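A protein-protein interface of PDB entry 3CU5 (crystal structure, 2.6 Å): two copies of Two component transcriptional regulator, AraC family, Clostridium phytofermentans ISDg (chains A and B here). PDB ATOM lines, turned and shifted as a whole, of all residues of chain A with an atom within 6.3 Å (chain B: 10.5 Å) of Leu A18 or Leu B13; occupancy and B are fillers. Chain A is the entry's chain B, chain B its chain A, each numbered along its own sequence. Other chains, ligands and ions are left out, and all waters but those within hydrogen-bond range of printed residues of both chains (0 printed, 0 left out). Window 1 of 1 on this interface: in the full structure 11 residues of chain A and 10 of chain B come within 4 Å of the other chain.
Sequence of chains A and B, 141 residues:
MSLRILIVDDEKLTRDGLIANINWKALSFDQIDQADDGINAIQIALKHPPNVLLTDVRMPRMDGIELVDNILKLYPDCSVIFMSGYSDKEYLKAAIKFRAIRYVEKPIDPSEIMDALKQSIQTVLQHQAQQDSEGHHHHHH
The side-chain carboxylate (OD2) of Asp B9 sits at hydrogen-bond distance from the backbone NH (N) of Glu B11, 3.0 Å away. NZ of Lys B12 is in salt-bridge range of OD1 of Asp B16, 3.1 Å away. The side-chain amide nitrogen of Asn B21 sits at hydrogen-bond distance from the backbone carbonyl oxygen of Gly B17, at 2.6 Å. O of Gly A17 is in hydrogen-bond range of ND2 of Asn A21 (2.6 Å).
Printed residues of chain B that touch a printed residue of chain A: Glu B11, Lys B12, Leu B13, Asp B16, Gly B17, Leu B18 and Asn B21. Of the 19 printed residues of chain A, 6 touch a printed residue of chain B. Among the printed residues, 12 pairs touch across the chains.
O of Leu A13 touches CA of Gly B17 (3.2 Å). Leu A13 touches Leu B18. Leu A13 touches Asn B21 (CD1 to ND2, 3.8 Å). O of Leu B13 touches CA of Gly A17 (3.2 Å). Gly A17 touches Gly B17 (N to CA, 3.7 Å). Leu A18 touches Leu B13 (CD2 to CD2, 3.6 Å). Ile A108 touches Leu B13.
Leu A13 touches Gly B17, and with the chains exchanged Gly A17 touches Leu B13. Leu A13 touches Leu B18, and with the chains exchanged Leu A18 touches Leu B13. Asp A16 touches Asn B21, and with the chains exchanged Asn A21 touches Asp B16. Gly A17 touches its own counterpart, Gly B17. Positions printed for both chains: 7, 13, 14, 15, 16, 17, 18, 19, 20, 21 and 83.
Of chain B, only Leu B13 comes within 4 Å of Leu A18. Leu B13 touches just these residues of chain A: Leu A13 (3.5 Å), Gly A17 (3.2 Å), Leu A18 (3.6 Å) and Ile A108 (3.9 Å). No residue of chain B comes within 4 Å of Thr A14. No residue of chain B comes within 4 Å of Ala A20. Of chain B, only Lys B12 (3.3 Å) and Asp B16 (2.8 Å) come within 4 Å of Asn A21. Printed residues of chain A within 4 Å of Leu B18: Leu A13. Of the printed residues of chain A, Lys B12 touches Asn A21. Of the printed residues of chain A, Glu B11 touches Ile A108. Asp B36 touches none of the printed residues of chain A. Leu A54 touches none of the printed residues of chain B. The nearest printed residue of chain B that does not touch Leu A13 is Thr B14 (4.1 Å).
NZ of Lys B12 is in hydrogen-bond range of OD1 of Asn A21, 3.3 Å away. The backbone NH (N) of Ile A108 sits at hydrogen-bond distance from the side-chain carboxylate (OE2) of Glu B11 (3.2 Å). OD1 of Asp B16 lies within hydrogen-bond range of ND2 of Asn A21 (2.8 Å). The backbone carbonyl oxygen (O) of Leu A13 lies close to the backbone carbonyl oxygen (O) of Leu B13 (3.5 Å). ND2 of Asn B21 sits at hydrogen-bond distance from OD1 of Asp A16 (3.1 Å).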
ATOM      1  N   ILE A   7       6.984 -13.991  20.578  1.00  0.00           N
ATOM      2  CA  ILE A   7       8.366 -13.567  20.183  1.00  0.00           C
ATOM      3  C   ILE A   7       8.297 -12.873  18.830  1.00  0.00           C
ATOM      4  O   ILE A   7       7.849 -13.476  17.860  1.00  0.00           O
ATOM      5  CB  ILE A   7       9.251 -14.789  20.106  1.00  0.00           C
ATOM      6  CG1 ILE A   7       9.228 -15.482  21.461  1.00  0.00           C
ATOM      7  CG2 ILE A   7      10.670 -14.462  19.700  1.00  0.00           C
ATOM      8  CD1 ILE A   7       9.866 -16.825  21.429  1.00  0.00           C
ATOM      9  N   LEU A  13      16.093 -15.977  11.168  1.00  0.00           N
ATOM     10  CA  LEU A  13      17.318 -16.516  11.680  1.00  0.00           C
ATOM     11  C   LEU A  13      17.383 -16.310  13.163  1.00  0.00           C
ATOM     12  O   LEU A  13      17.933 -17.143  13.873  1.00  0.00           O
ATOM     13  CB  LEU A  13      18.497 -15.823  11.045  1.00  0.00           C
ATOM     14  CG  LEU A  13      19.214 -16.686  10.022  1.00  0.00           C
ATOM     15  CD1 LEU A  13      18.231 -17.325   9.083  1.00  0.00           C
ATOM     16  CD2 LEU A  13      20.232 -15.800   9.308  1.00  0.00           C
ATOM     17  N   THR A  14      16.818 -15.207  13.640  1.00  0.00           N
ATOM     18  CA  THR A  14      17.027 -14.828  15.016  1.00  0.00           C
ATOM     19  C   THR A  14      15.992 -15.449  15.968  1.00  0.00           C
ATOM     20  O   THR A  14      16.324 -15.943  17.045  1.00  0.00           O
ATOM     21  CB  THR A  14      17.049 -13.294  15.183  1.00  0.00           C
ATOM     22  OG1 THR A  14      18.164 -12.737  14.457  1.00  0.00           O
ATOM     23  CG2 THR A  14      17.193 -12.952  16.667  1.00  0.00           C
ATOM     24  N   ARG A  15      14.724 -15.408  15.598  1.00  0.00           N
ATOM     25  CA  ARG A  15      13.762 -16.079  16.444  1.00  0.00           C
ATOM     26  C   ARG A  15      14.128 -17.573  16.601  1.00  0.00           C
ATOM     27  O   ARG A  15      14.017 -18.143  17.702  1.00  0.00           O
ATOM     28  CB  ARG A  15      12.420 -16.005  15.796  1.00  0.00           C
ATOM     29  CG  ARG A  15      11.857 -14.653  15.614  1.00  0.00           C
ATOM     30  CD  ARG A  15      10.489 -14.940  14.953  1.00  0.00           C
ATOM     31  NE  ARG A  15      10.423 -14.136  13.780  1.00  0.00           N
ATOM     32  CZ  ARG A  15      10.057 -14.551  12.598  1.00  0.00           C
ATOM     33  NH1 ARG A  15       9.660 -15.800  12.406  1.00  0.00           N
ATOM     34  NH2 ARG A  15      10.071 -13.658  11.600  1.00  0.00           N
ATOM     35  N   ASP A  16      14.540 -18.201  15.493  1.00  0.00           N
ATOM     36  CA  ASP A  16      14.998 -19.583  15.517  1.00  0.00           C
ATOM     37  C   ASP A  16      16.240 -19.786  16.398  1.00  0.00           C
ATOM     38  O   ASP A  16      16.276 -20.733  17.185  1.00  0.00           O
ATOM     39  CB  ASP A  16      15.273 -20.096  14.111  1.00  0.00           C
ATOM     40  CG  ASP A  16      13.982 -20.434  13.335  1.00  0.00           C
ATOM     41  OD1 ASP A  16      14.096 -20.828  12.116  1.00  0.00           O
ATOM     42  OD2 ASP A  16      12.870 -20.329  13.952  1.00  0.00           O
ATOM     43  N   GLY A  17      17.268 -18.933  16.271  1.00  0.00           N
ATOM     44  CA  GLY A  17      18.414 -19.041  17.180  1.00  0.00           C
ATOM     45  C   GLY A  17      17.909 -18.924  18.608  1.00  0.00           C
ATOM     46  O   GLY A  17      18.233 -19.713  19.487  1.00  0.00           O
ATOM     47  N   LEU A  18      17.090 -17.915  18.821  1.00  0.00           N
ATOM     48  CA  LEU A  18      16.515 -17.620  20.129  1.00  0.00           C
ATOM     49  C   LEU A  18      15.793 -18.850  20.771  1.00  0.00           C
ATOM     50  O   LEU A  18      16.086 -19.257  21.917  1.00  0.00           O
ATOM     51  CB  LEU A  18      15.555 -16.427  19.957  1.00  0.00           C
ATOM     52  CG  LEU A  18      15.031 -15.566  21.101  1.00  0.00           C
ATOM     53  CD1 LEU A  18      14.179 -16.436  22.037  1.00  0.00           C
ATOM     54  CD2 LEU A  18      16.148 -14.831  21.877  1.00  0.00           C
ATOM     55  N   ILE A  19      14.859 -19.432  20.027  1.00  0.00           N
ATOM     56  CA  ILE A  19      14.104 -20.557  20.509  1.00  0.00           C
ATOM     57  C   ILE A  19      15.026 -21.722  20.733  1.00  0.00           C
ATOM     58  O   ILE A  19      14.955 -22.437  21.730  1.00  0.00           O
ATOM     59  CB  ILE A  19      13.053 -20.939  19.478  1.00  0.00           C
ATOM     60  CG1 ILE A  19      12.024 -19.780  19.395  1.00  0.00           C
ATOM     61  CG2 ILE A  19      12.344 -22.192  19.901  1.00  0.00           C
ATOM     62  CD1 ILE A  19      11.371 -19.667  18.095  1.00  0.00           C
ATOM     63  N   ALA A  20      15.935 -21.895  19.790  1.00  0.00           N
ATOM     64  CA  ALA A  20      16.848 -23.039  19.823  1.00  0.00           C
ATOM     65  C   ALA A  20      17.669 -22.988  21.111  1.00  0.00           C
ATOM     66  O   ALA A  20      18.099 -24.033  21.640  1.00  0.00           O
ATOM     67  CB  ALA A  20      17.760 -22.997  18.628  1.00  0.00           C
ATOM     68  N   ASN A  21      17.885 -21.774  21.618  1.00  0.00           N
ATOM     69  CA  ASN A  21      18.817 -21.581  22.729  1.00  0.00           C
ATOM     70  C   ASN A  21      18.160 -21.446  24.091  1.00  0.00           C
ATOM     71  O   ASN A  21      18.828 -21.263  25.085  1.00  0.00           O
ATOM     72  CB  ASN A  21      19.707 -20.384  22.443  1.00  0.00           C
ATOM     73  CG  ASN A  21      20.832 -20.736  21.491  1.00  0.00           C
ATOM     74  OD1 ASN A  21      21.825 -21.315  21.913  1.00  0.00           O
ATOM     75  ND2 ASN A  21      20.674 -20.417  20.195  1.00  0.00           N
ATOM     76  N   ILE A  22      16.842 -21.523  24.137  1.00  0.00           N
ATOM     77  CA  ILE A  22      16.157 -21.341  25.379  1.00  0.00           C
ATOM     78  C   ILE A  22      15.745 -22.707  25.760  1.00  0.00           C
ATOM     79  O   ILE A  22      15.429 -23.538  24.911  1.00  0.00           O
ATOM     80  CB  ILE A  22      14.911 -20.515  25.204  1.00  0.00           C
ATOM     81  CG1 ILE A  22      15.281 -19.095  24.772  1.00  0.00           C
ATOM     82  CG2 ILE A  22      14.138 -20.461  26.484  1.00  0.00           C
ATOM     83  CD1 ILE A  22      14.011 -18.294  24.244  1.00  0.00           C
ATOM     84  N   TRP A  24      12.890 -24.352  27.164  1.00  0.00           N
ATOM     85  CA  TRP A  24      11.491 -24.142  27.467  1.00  0.00           C
ATOM     86  C   TRP A  24      11.013 -25.126  28.504  1.00  0.00           C
ATOM     87  O   TRP A  24       9.970 -24.914  29.123  1.00  0.00           O
ATOM     88  CB  TRP A  24      10.679 -24.275  26.185  1.00  0.00           C
ATOM     89  CG  TRP A  24      11.247 -23.374  25.106  1.00  0.00           C
ATOM     90  CD1 TRP A  24      12.004 -23.751  24.008  1.00  0.00           C
ATOM     91  CD2 TRP A  24      11.122 -21.927  25.030  1.00  0.00           C
ATOM     92  NE1 TRP A  24      12.345 -22.633  23.265  1.00  0.00           N
ATOM     93  CE2 TRP A  24      11.833 -21.506  23.869  1.00  0.00           C
ATOM     94  CE3 TRP A  24      10.482 -20.957  25.827  1.00  0.00           C
ATOM     95  CZ2 TRP A  24      11.922 -20.155  23.493  1.00  0.00           C
ATOM     96  CZ3 TRP A  24      10.576 -19.608  25.452  1.00  0.00           C
ATOM     97  CH2 TRP A  24      11.298 -19.222  24.301  1.00  0.00           C
ATOM     98  N   LEU A  54       8.377 -10.555  23.567  1.00  0.00           N
ATOM     99  CA  LEU A  54       9.812 -10.396  23.426  1.00  0.00           C
ATOM    100  C   LEU A  54      10.079  -9.784  22.062  1.00  0.00           C
ATOM    101  O   LEU A  54       9.647 -10.307  21.022  1.00  0.00           O
ATOM    102  CB  LEU A  54      10.461 -11.753  23.497  1.00  0.00           C
ATOM    103  CG  LEU A  54      11.908 -11.869  23.941  1.00  0.00           C
ATOM    104  CD1 LEU A  54      12.221 -13.360  23.968  1.00  0.00           C
ATOM    105  CD2 LEU A  54      12.876 -11.112  23.010  1.00  0.00           C
ATOM    106  N   MET A  83      14.955  -6.879  23.008  1.00  0.00           N
ATOM    107  CA  MET A  83      16.336  -7.160  22.686  1.00  0.00           C
ATOM    108  C   MET A  83      16.849  -5.880  22.070  1.00  0.00           C
ATOM    109  O   MET A  83      16.388  -5.479  21.012  1.00  0.00           O
ATOM    110  CB  MET A  83      16.445  -8.331  21.718  1.00  0.00           C
ATOM    111  CG  MET A  83      15.928  -9.638  22.315  1.00  0.00           C
ATOM    112  SD  MET A  83      15.577 -10.958  21.105  1.00  0.00           S
ATOM    113  CE  MET A  83      14.070 -10.441  20.227  1.00  0.00           C
ATOM    114  N   ILE A 108      23.107 -10.740  21.951  1.00  0.00           N
ATOM    115  CA  ILE A 108      22.365 -11.416  23.005  1.00  0.00           C
ATOM    116  C   ILE A 108      23.166 -12.539  23.588  1.00  0.00           C
ATOM    117  O   ILE A 108      23.766 -13.334  22.882  1.00  0.00           O
ATOM    118  CB  ILE A 108      20.999 -12.003  22.590  1.00  0.00           C
ATOM    119  CG1 ILE A 108      19.976 -10.882  22.390  1.00  0.00           C
ATOM    120  CG2 ILE A 108      20.490 -12.924  23.708  1.00  0.00           C
ATOM    121  CD1 ILE A 108      19.452 -10.836  21.003  1.00  0.00           C
ATOM    122  N   ASP A 109      23.182 -12.597  24.905  1.00  0.00           N
ATOM    123  CA  ASP A 109      23.681 -13.759  25.649  1.00  0.00           C
ATOM    124  C   ASP A 109      22.400 -14.494  26.088  1.00  0.00           C
ATOM    125  O   ASP A 109      21.490 -13.875  26.693  1.00  0.00           O
ATOM    126  CB  ASP A 109      24.527 -13.273  26.826  1.00  0.00           C
ATOM    127  CG  ASP A 109      24.901 -14.375  27.791  1.00  0.00           C
ATOM    128  OD1 ASP A 109      25.837 -14.141  28.592  1.00  0.00           O
ATOM    129  OD2 ASP A 109      24.281 -15.456  27.778  1.00  0.00           O
ATOM    130  N   PRO A 110      22.301 -15.797  25.745  1.00  0.00           N
ATOM    131  CA  PRO A 110      21.094 -16.599  26.017  1.00  0.00           C
ATOM    132  C   PRO A 110      20.961 -16.983  27.490  1.00  0.00           C
ATOM    133  O   PRO A 110      20.079 -17.731  27.866  1.00  0.00           O
ATOM    134  CB  PRO A 110      21.286 -17.852  25.144  1.00  0.00           C
ATOM    135  CG  PRO A 110      22.662 -17.674  24.432  1.00  0.00           C
ATOM    136  CD  PRO A 110      23.397 -16.629  25.209  1.00  0.00           C
ATOM    137  N   ILE A 113      18.931 -13.643  28.493  1.00  0.00           N
ATOM    138  CA  ILE A 113      17.593 -13.912  28.097  1.00  0.00           C
ATOM    139  C   ILE A 113      16.865 -14.973  28.888  1.00  0.00           C
ATOM    140  O   ILE A 113      15.665 -15.017  28.821  1.00  0.00           O
ATOM    141  CB  ILE A 113      17.509 -14.353  26.673  1.00  0.00           C
ATOM    142  CG1 ILE A 113      16.729 -13.329  25.899  1.00  0.00           C
ATOM    143  CG2 ILE A 113      16.692 -15.585  26.584  1.00  0.00           C
ATOM    144  CD1 ILE A 113      17.364 -13.094  24.567  1.00  0.00           C
ATOM    145  N   LEU A 117      13.453 -14.007  31.166  1.00  0.00           N
ATOM    146  CA  LEU A 117      12.216 -14.798  31.054  1.00  0.00           C
ATOM    147  C   LEU A 117      11.725 -15.344  32.413  1.00  0.00           C
ATOM    148  O   LEU A 117      10.515 -15.329  32.708  1.00  0.00           O
ATOM    149  CB  LEU A 117      12.315 -15.911  30.015  1.00  0.00           C
ATOM    150  CG  LEU A 117      12.542 -15.678  28.513  1.00  0.00           C
ATOM    151  CD1 LEU A 117      12.960 -17.021  27.956  1.00  0.00           C
ATOM    152  CD2 LEU A 117      11.393 -15.084  27.655  1.00  0.00           C
ATOM    153  N   ILE B   7      31.346 -19.590   8.712  1.00  0.00           N
ATOM    154  CA  ILE B   7      30.253 -18.692   9.021  1.00  0.00           C
ATOM    155  C   ILE B   7      30.738 -17.729  10.070  1.00  0.00           C
ATOM    156  O   ILE B   7      31.183 -18.118  11.159  1.00  0.00           O
ATOM    157  CB  ILE B   7      29.135 -19.468   9.664  1.00  0.00           C
ATOM    158  CG1 ILE B   7      28.558 -20.460   8.682  1.00  0.00           C
ATOM    159  CG2 ILE B   7      28.069 -18.538  10.232  1.00  0.00           C
ATOM    160  CD1 ILE B   7      27.439 -21.275   9.322  1.00  0.00           C
ATOM    161  N   VAL B   8      30.673 -16.458   9.763  1.00  0.00           N
ATOM    162  CA  VAL B   8      31.236 -15.501  10.682  1.00  0.00           C
ATOM    163  C   VAL B   8      30.227 -14.442  11.121  1.00  0.00           C
ATOM    164  O   VAL B   8      29.776 -13.610  10.327  1.00  0.00           O
ATOM    165  CB  VAL B   8      32.444 -14.813  10.111  1.00  0.00           C
ATOM    166  CG1 VAL B   8      32.985 -13.859  11.131  1.00  0.00           C
ATOM    167  CG2 VAL B   8      33.482 -15.819   9.749  1.00  0.00           C
ATOM    168  N   ASP B   9      29.876 -14.490  12.402  1.00  0.00           N
ATOM    169  CA  ASP B   9      28.946 -13.540  12.917  1.00  0.00           C
ATOM    170  C   ASP B   9      29.125 -13.316  14.392  1.00  0.00           C
ATOM    171  O   ASP B   9      29.337 -14.248  15.182  1.00  0.00           O
ATOM    172  CB  ASP B   9      27.527 -13.970  12.635  1.00  0.00           C
ATOM    173  CG  ASP B   9      26.569 -12.791  12.607  1.00  0.00           C
ATOM    174  OD1 ASP B   9      26.360 -12.256  11.497  1.00  0.00           O
ATOM    175  OD2 ASP B   9      26.026 -12.397  13.670  1.00  0.00           O
ATOM    176  N   ASP B  10      29.030 -12.042  14.736  1.00  0.00           N
ATOM    177  CA  ASP B  10      29.075 -11.532  16.087  1.00  0.00           C
ATOM    178  C   ASP B  10      28.123 -12.284  17.056  1.00  0.00           C
ATOM    179  O   ASP B  10      28.474 -12.521  18.213  1.00  0.00           O
ATOM    180  CB  ASP B  10      28.700 -10.046  16.001  1.00  0.00           C
ATOM    181  CG  ASP B  10      28.888  -9.337  17.307  1.00  0.00           C
ATOM    182  OD1 ASP B  10      28.438  -8.173  17.482  1.00  0.00           O
ATOM    183  OD2 ASP B  10      29.507  -9.976  18.180  1.00  0.00           O
ATOM    184  N   GLU B  11      26.939 -12.684  16.565  1.00  0.00           N
ATOM    185  CA  GLU B  11      25.854 -13.166  17.422  1.00  0.00           C
ATOM    186  C   GLU B  11      25.521 -14.638  17.307  1.00  0.00           C
ATOM    187  O   GLU B  11      25.081 -15.103  16.257  1.00  0.00           O
ATOM    188  CB  GLU B  11      24.562 -12.374  17.183  1.00  0.00           C
ATOM    189  CG  GLU B  11      23.545 -12.553  18.321  1.00  0.00           C
ATOM    190  CD  GLU B  11      22.826 -11.253  18.661  1.00  0.00           C
ATOM    191  OE1 GLU B  11      21.562 -11.255  18.714  1.00  0.00           O
ATOM    192  OE2 GLU B  11      23.523 -10.228  18.864  1.00  0.00           O
ATOM    193  N   LYS B  12      25.664 -15.333  18.436  1.00  0.00           N
ATOM    194  CA  LYS B  12      25.421 -16.755  18.548  1.00  0.00           C
ATOM    195  C   LYS B  12      24.053 -17.180  17.983  1.00  0.00           C
ATOM    196  O   LYS B  12      23.921 -18.218  17.285  1.00  0.00           O
ATOM    197  CB  LYS B  12      25.513 -17.144  20.010  1.00  0.00           C
ATOM    198  CG  LYS B  12      25.415 -18.627  20.268  1.00  0.00           C
ATOM    199  CD  LYS B  12      25.564 -18.893  21.770  1.00  0.00           C
ATOM    200  CE  LYS B  12      25.814 -20.377  22.081  1.00  0.00           C
ATOM    201  NZ  LYS B  12      25.025 -21.304  21.193  1.00  0.00           N
ATOM    202  N   LEU B  13      23.033 -16.376  18.268  1.00  0.00           N
ATOM    203  CA  LEU B  13      21.696 -16.676  17.850  1.00  0.00           C
ATOM    204  C   LEU B  13      21.580 -16.636  16.355  1.00  0.00           C
ATOM    205  O   LEU B  13      20.802 -17.398  15.777  1.00  0.00           O
ATOM    206  CB  LEU B  13      20.730 -15.690  18.481  1.00  0.00           C
ATOM    207  CG  LEU B  13      20.137 -16.009  19.859  1.00  0.00           C
ATOM    208  CD1 LEU B  13      21.204 -16.399  20.855  1.00  0.00           C
ATOM    209  CD2 LEU B  13      19.378 -14.818  20.344  1.00  0.00           C
ATOM    210  N   THR B  14      22.360 -15.780  15.696  1.00  0.00           N
ATOM    211  CA  THR B  14      22.297 -15.740  14.207  1.00  0.00           C
ATOM    212  C   THR B  14      22.988 -16.868  13.478  1.00  0.00           C
ATOM    213  O   THR B  14      22.499 -17.294  12.443  1.00  0.00           O
ATOM    214  CB  THR B  14      22.972 -14.525  13.638  1.00  0.00           C
ATOM    215  OG1 THR B  14      22.356 -13.334  14.160  1.00  0.00           O
ATOM    216  CG2 THR B  14      22.941 -14.560  12.087  1.00  0.00           C
ATOM    217  N   ARG B  15      24.159 -17.299  13.968  1.00  0.00           N
ATOM    218  CA  ARG B  15      24.840 -18.500  13.458  1.00  0.00           C
ATOM    219  C   ARG B  15      23.962 -19.741  13.664  1.00  0.00           C
ATOM    220  O   ARG B  15      23.476 -20.331  12.719  1.00  0.00           O
ATOM    221  CB  ARG B  15      26.110 -18.701  14.267  1.00  0.00           C
ATOM    222  CG  ARG B  15      27.255 -17.796  13.917  1.00  0.00           C
ATOM    223  CD  ARG B  15      28.433 -18.231  14.750  1.00  0.00           C
ATOM    224  NE  ARG B  15      28.697 -17.281  15.825  1.00  0.00           N
ATOM    225  CZ  ARG B  15      28.856 -17.577  17.115  1.00  0.00           C
ATOM    226  NH1 ARG B  15      28.792 -18.822  17.546  1.00  0.00           N
ATOM    227  NH2 ARG B  15      29.092 -16.591  17.973  1.00  0.00           N
ATOM    228  N   ASP B  16      23.781 -20.138  14.920  1.00  0.00           N
ATOM    229  CA  ASP B  16      22.740 -21.087  15.281  1.00  0.00           C
ATOM    230  C   ASP B  16      21.524 -21.053  14.349  1.00  0.00           C
ATOM    231  O   ASP B  16      21.209 -22.073  13.737  1.00  0.00           O
ATOM    232  CB  ASP B  16      22.276 -20.873  16.719  1.00  0.00           C
ATOM    233  CG  ASP B  16      23.289 -21.366  17.733  1.00  0.00           C
ATOM    234  OD1 ASP B  16      22.956 -21.549  18.944  1.00  0.00           O
ATOM    235  OD2 ASP B  16      24.438 -21.580  17.305  1.00  0.00           O
ATOM    236  N   GLY B  17      20.817 -19.928  14.240  1.00  0.00           N
ATOM    237  CA  GLY B  17      19.505 -19.923  13.531  1.00  0.00           C
ATOM    238  C   GLY B  17      19.774 -20.155  12.058  1.00  0.00           C
ATOM    239  O   GLY B  17      18.988 -20.699  11.311  1.00  0.00           O
ATOM    240  N   LEU B  18      20.945 -19.747  11.634  1.00  0.00           N
ATOM    241  CA  LEU B  18      21.370 -20.000  10.276  1.00  0.00           C
ATOM    242  C   LEU B  18      21.622 -21.457  10.061  1.00  0.00           C
ATOM    243  O   LEU B  18      21.069 -22.080   9.179  1.00  0.00           O
ATOM    244  CB  LEU B  18      22.690 -19.307  10.065  1.00  0.00           C
ATOM    245  CG  LEU B  18      22.673 -18.931   8.624  1.00  0.00           C
ATOM    246  CD1 LEU B  18      23.438 -17.639   8.494  1.00  0.00           C
ATOM    247  CD2 LEU B  18      23.304 -20.122   7.934  1.00  0.00           C
ATOM    248  N   ILE B  19      22.494 -22.009  10.873  1.00  0.00           N
ATOM    249  CA  ILE B  19      22.754 -23.383  10.735  1.00  0.00           C
ATOM    250  C   ILE B  19      21.439 -24.148  10.825  1.00  0.00           C
ATOM    251  O   ILE B  19      21.180 -25.019  10.028  1.00  0.00           O
ATOM    252  CB  ILE B  19      23.736 -23.801  11.788  1.00  0.00           C
ATOM    253  CG1 ILE B  19      25.169 -23.480  11.289  1.00  0.00           C
ATOM    254  CG2 ILE B  19      23.604 -25.231  12.038  1.00  0.00           C
ATOM    255  CD1 ILE B  19      26.175 -23.251  12.412  1.00  0.00           C
ATOM    256  N   ALA B  20      20.578 -23.794  11.770  1.00  0.00           N
ATOM    257  CA  ALA B  20      19.278 -24.456  11.897  1.00  0.00           C
ATOM    258  C   ALA B  20      18.493 -24.449  10.592  1.00  0.00           C
ATOM    259  O   ALA B  20      17.759 -25.396  10.284  1.00  0.00           O
ATOM    260  CB  ALA B  20      18.461 -23.799  12.980  1.00  0.00           C
ATOM    261  N   ASN B  21      18.650 -23.376   9.823  1.00  0.00           N
ATOM    262  CA  ASN B  21      17.841 -23.168   8.644  1.00  0.00           C
ATOM    263  C   ASN B  21      18.443 -23.694   7.368  1.00  0.00           C
ATOM    264  O   ASN B  21      17.851 -23.525   6.319  1.00  0.00           O
ATOM    265  CB  ASN B  21      17.564 -21.685   8.457  1.00  0.00           C
ATOM    266  CG  ASN B  21      16.359 -21.223   9.239  1.00  0.00           C
ATOM    267  OD1 ASN B  21      15.219 -21.473   8.829  1.00  0.00           O
ATOM    268  ND2 ASN B  21      16.591 -20.541  10.364  1.00  0.00           N
ATOM    269  N   GLN B  34      32.635 -21.957  12.478  1.00  0.00           N
ATOM    270  CA  GLN B  34      32.207 -20.643  12.943  1.00  0.00           C
ATOM    271  C   GLN B  34      32.959 -20.131  14.172  1.00  0.00           C
ATOM    272  O   GLN B  34      33.663 -20.888  14.809  1.00  0.00           O
ATOM    273  CB  GLN B  34      30.755 -20.771  13.391  1.00  0.00           C
ATOM    274  CG  GLN B  34      30.495 -21.919  14.345  1.00  0.00           C
ATOM    275  CD  GLN B  34      29.015 -22.256  14.420  1.00  0.00           C
ATOM    276  OE1 GLN B  34      28.621 -23.201  15.043  1.00  0.00           O
ATOM    277  NE2 GLN B  34      28.206 -21.491  13.756  1.00  0.00           N
ATOM    278  N   ALA B  35      32.931 -18.850  14.520  1.00  0.00           N
ATOM    279  CA  ALA B  35      33.847 -17.743  14.210  1.00  0.00           C
ATOM    280  C   ALA B  35      33.038 -16.475  14.409  1.00  0.00           C
ATOM    281  O   ALA B  35      32.065 -16.236  13.731  1.00  0.00           O
ATOM    282  CB  ALA B  35      34.637 -17.797  12.911  1.00  0.00           C
ATOM    283  N   ASP B  36      33.390 -15.735  15.445  1.00  0.00           N
ATOM    284  CA  ASP B  36      32.557 -14.658  15.941  1.00  0.00           C
ATOM    285  C   ASP B  36      33.064 -13.271  15.532  1.00  0.00           C
ATOM    286  O   ASP B  36      32.359 -12.269  15.681  1.00  0.00           O
ATOM    287  CB  ASP B  36      32.552 -14.690  17.457  1.00  0.00           C
ATOM    288  CG  ASP B  36      33.572 -13.755  18.024  1.00  0.00           C
ATOM    289  OD1 ASP B  36      34.587 -13.480  17.317  1.00  0.00           O
ATOM    290  OD2 ASP B  36      33.347 -13.272  19.162  1.00  0.00           O
ATOM    291  N   MET B  83      25.974 -11.087   4.144  1.00  0.00           N
ATOM    292  CA  MET B  83      24.673 -10.655   4.565  1.00  0.00           C
ATOM    293  C   MET B  83      24.782  -9.126   4.782  1.00  0.00           C
ATOM    294  O   MET B  83      25.720  -8.656   5.441  1.00  0.00           O
ATOM    295  CB  MET B  83      24.274 -11.436   5.813  1.00  0.00           C
ATOM    296  CG  MET B  83      24.390 -12.942   5.614  1.00  0.00           C
ATOM    297  SD  MET B  83      24.236 -13.895   7.162  1.00  0.00           S
ATOM    298  CE  MET B  83      25.866 -13.481   7.887  1.00  0.00           C
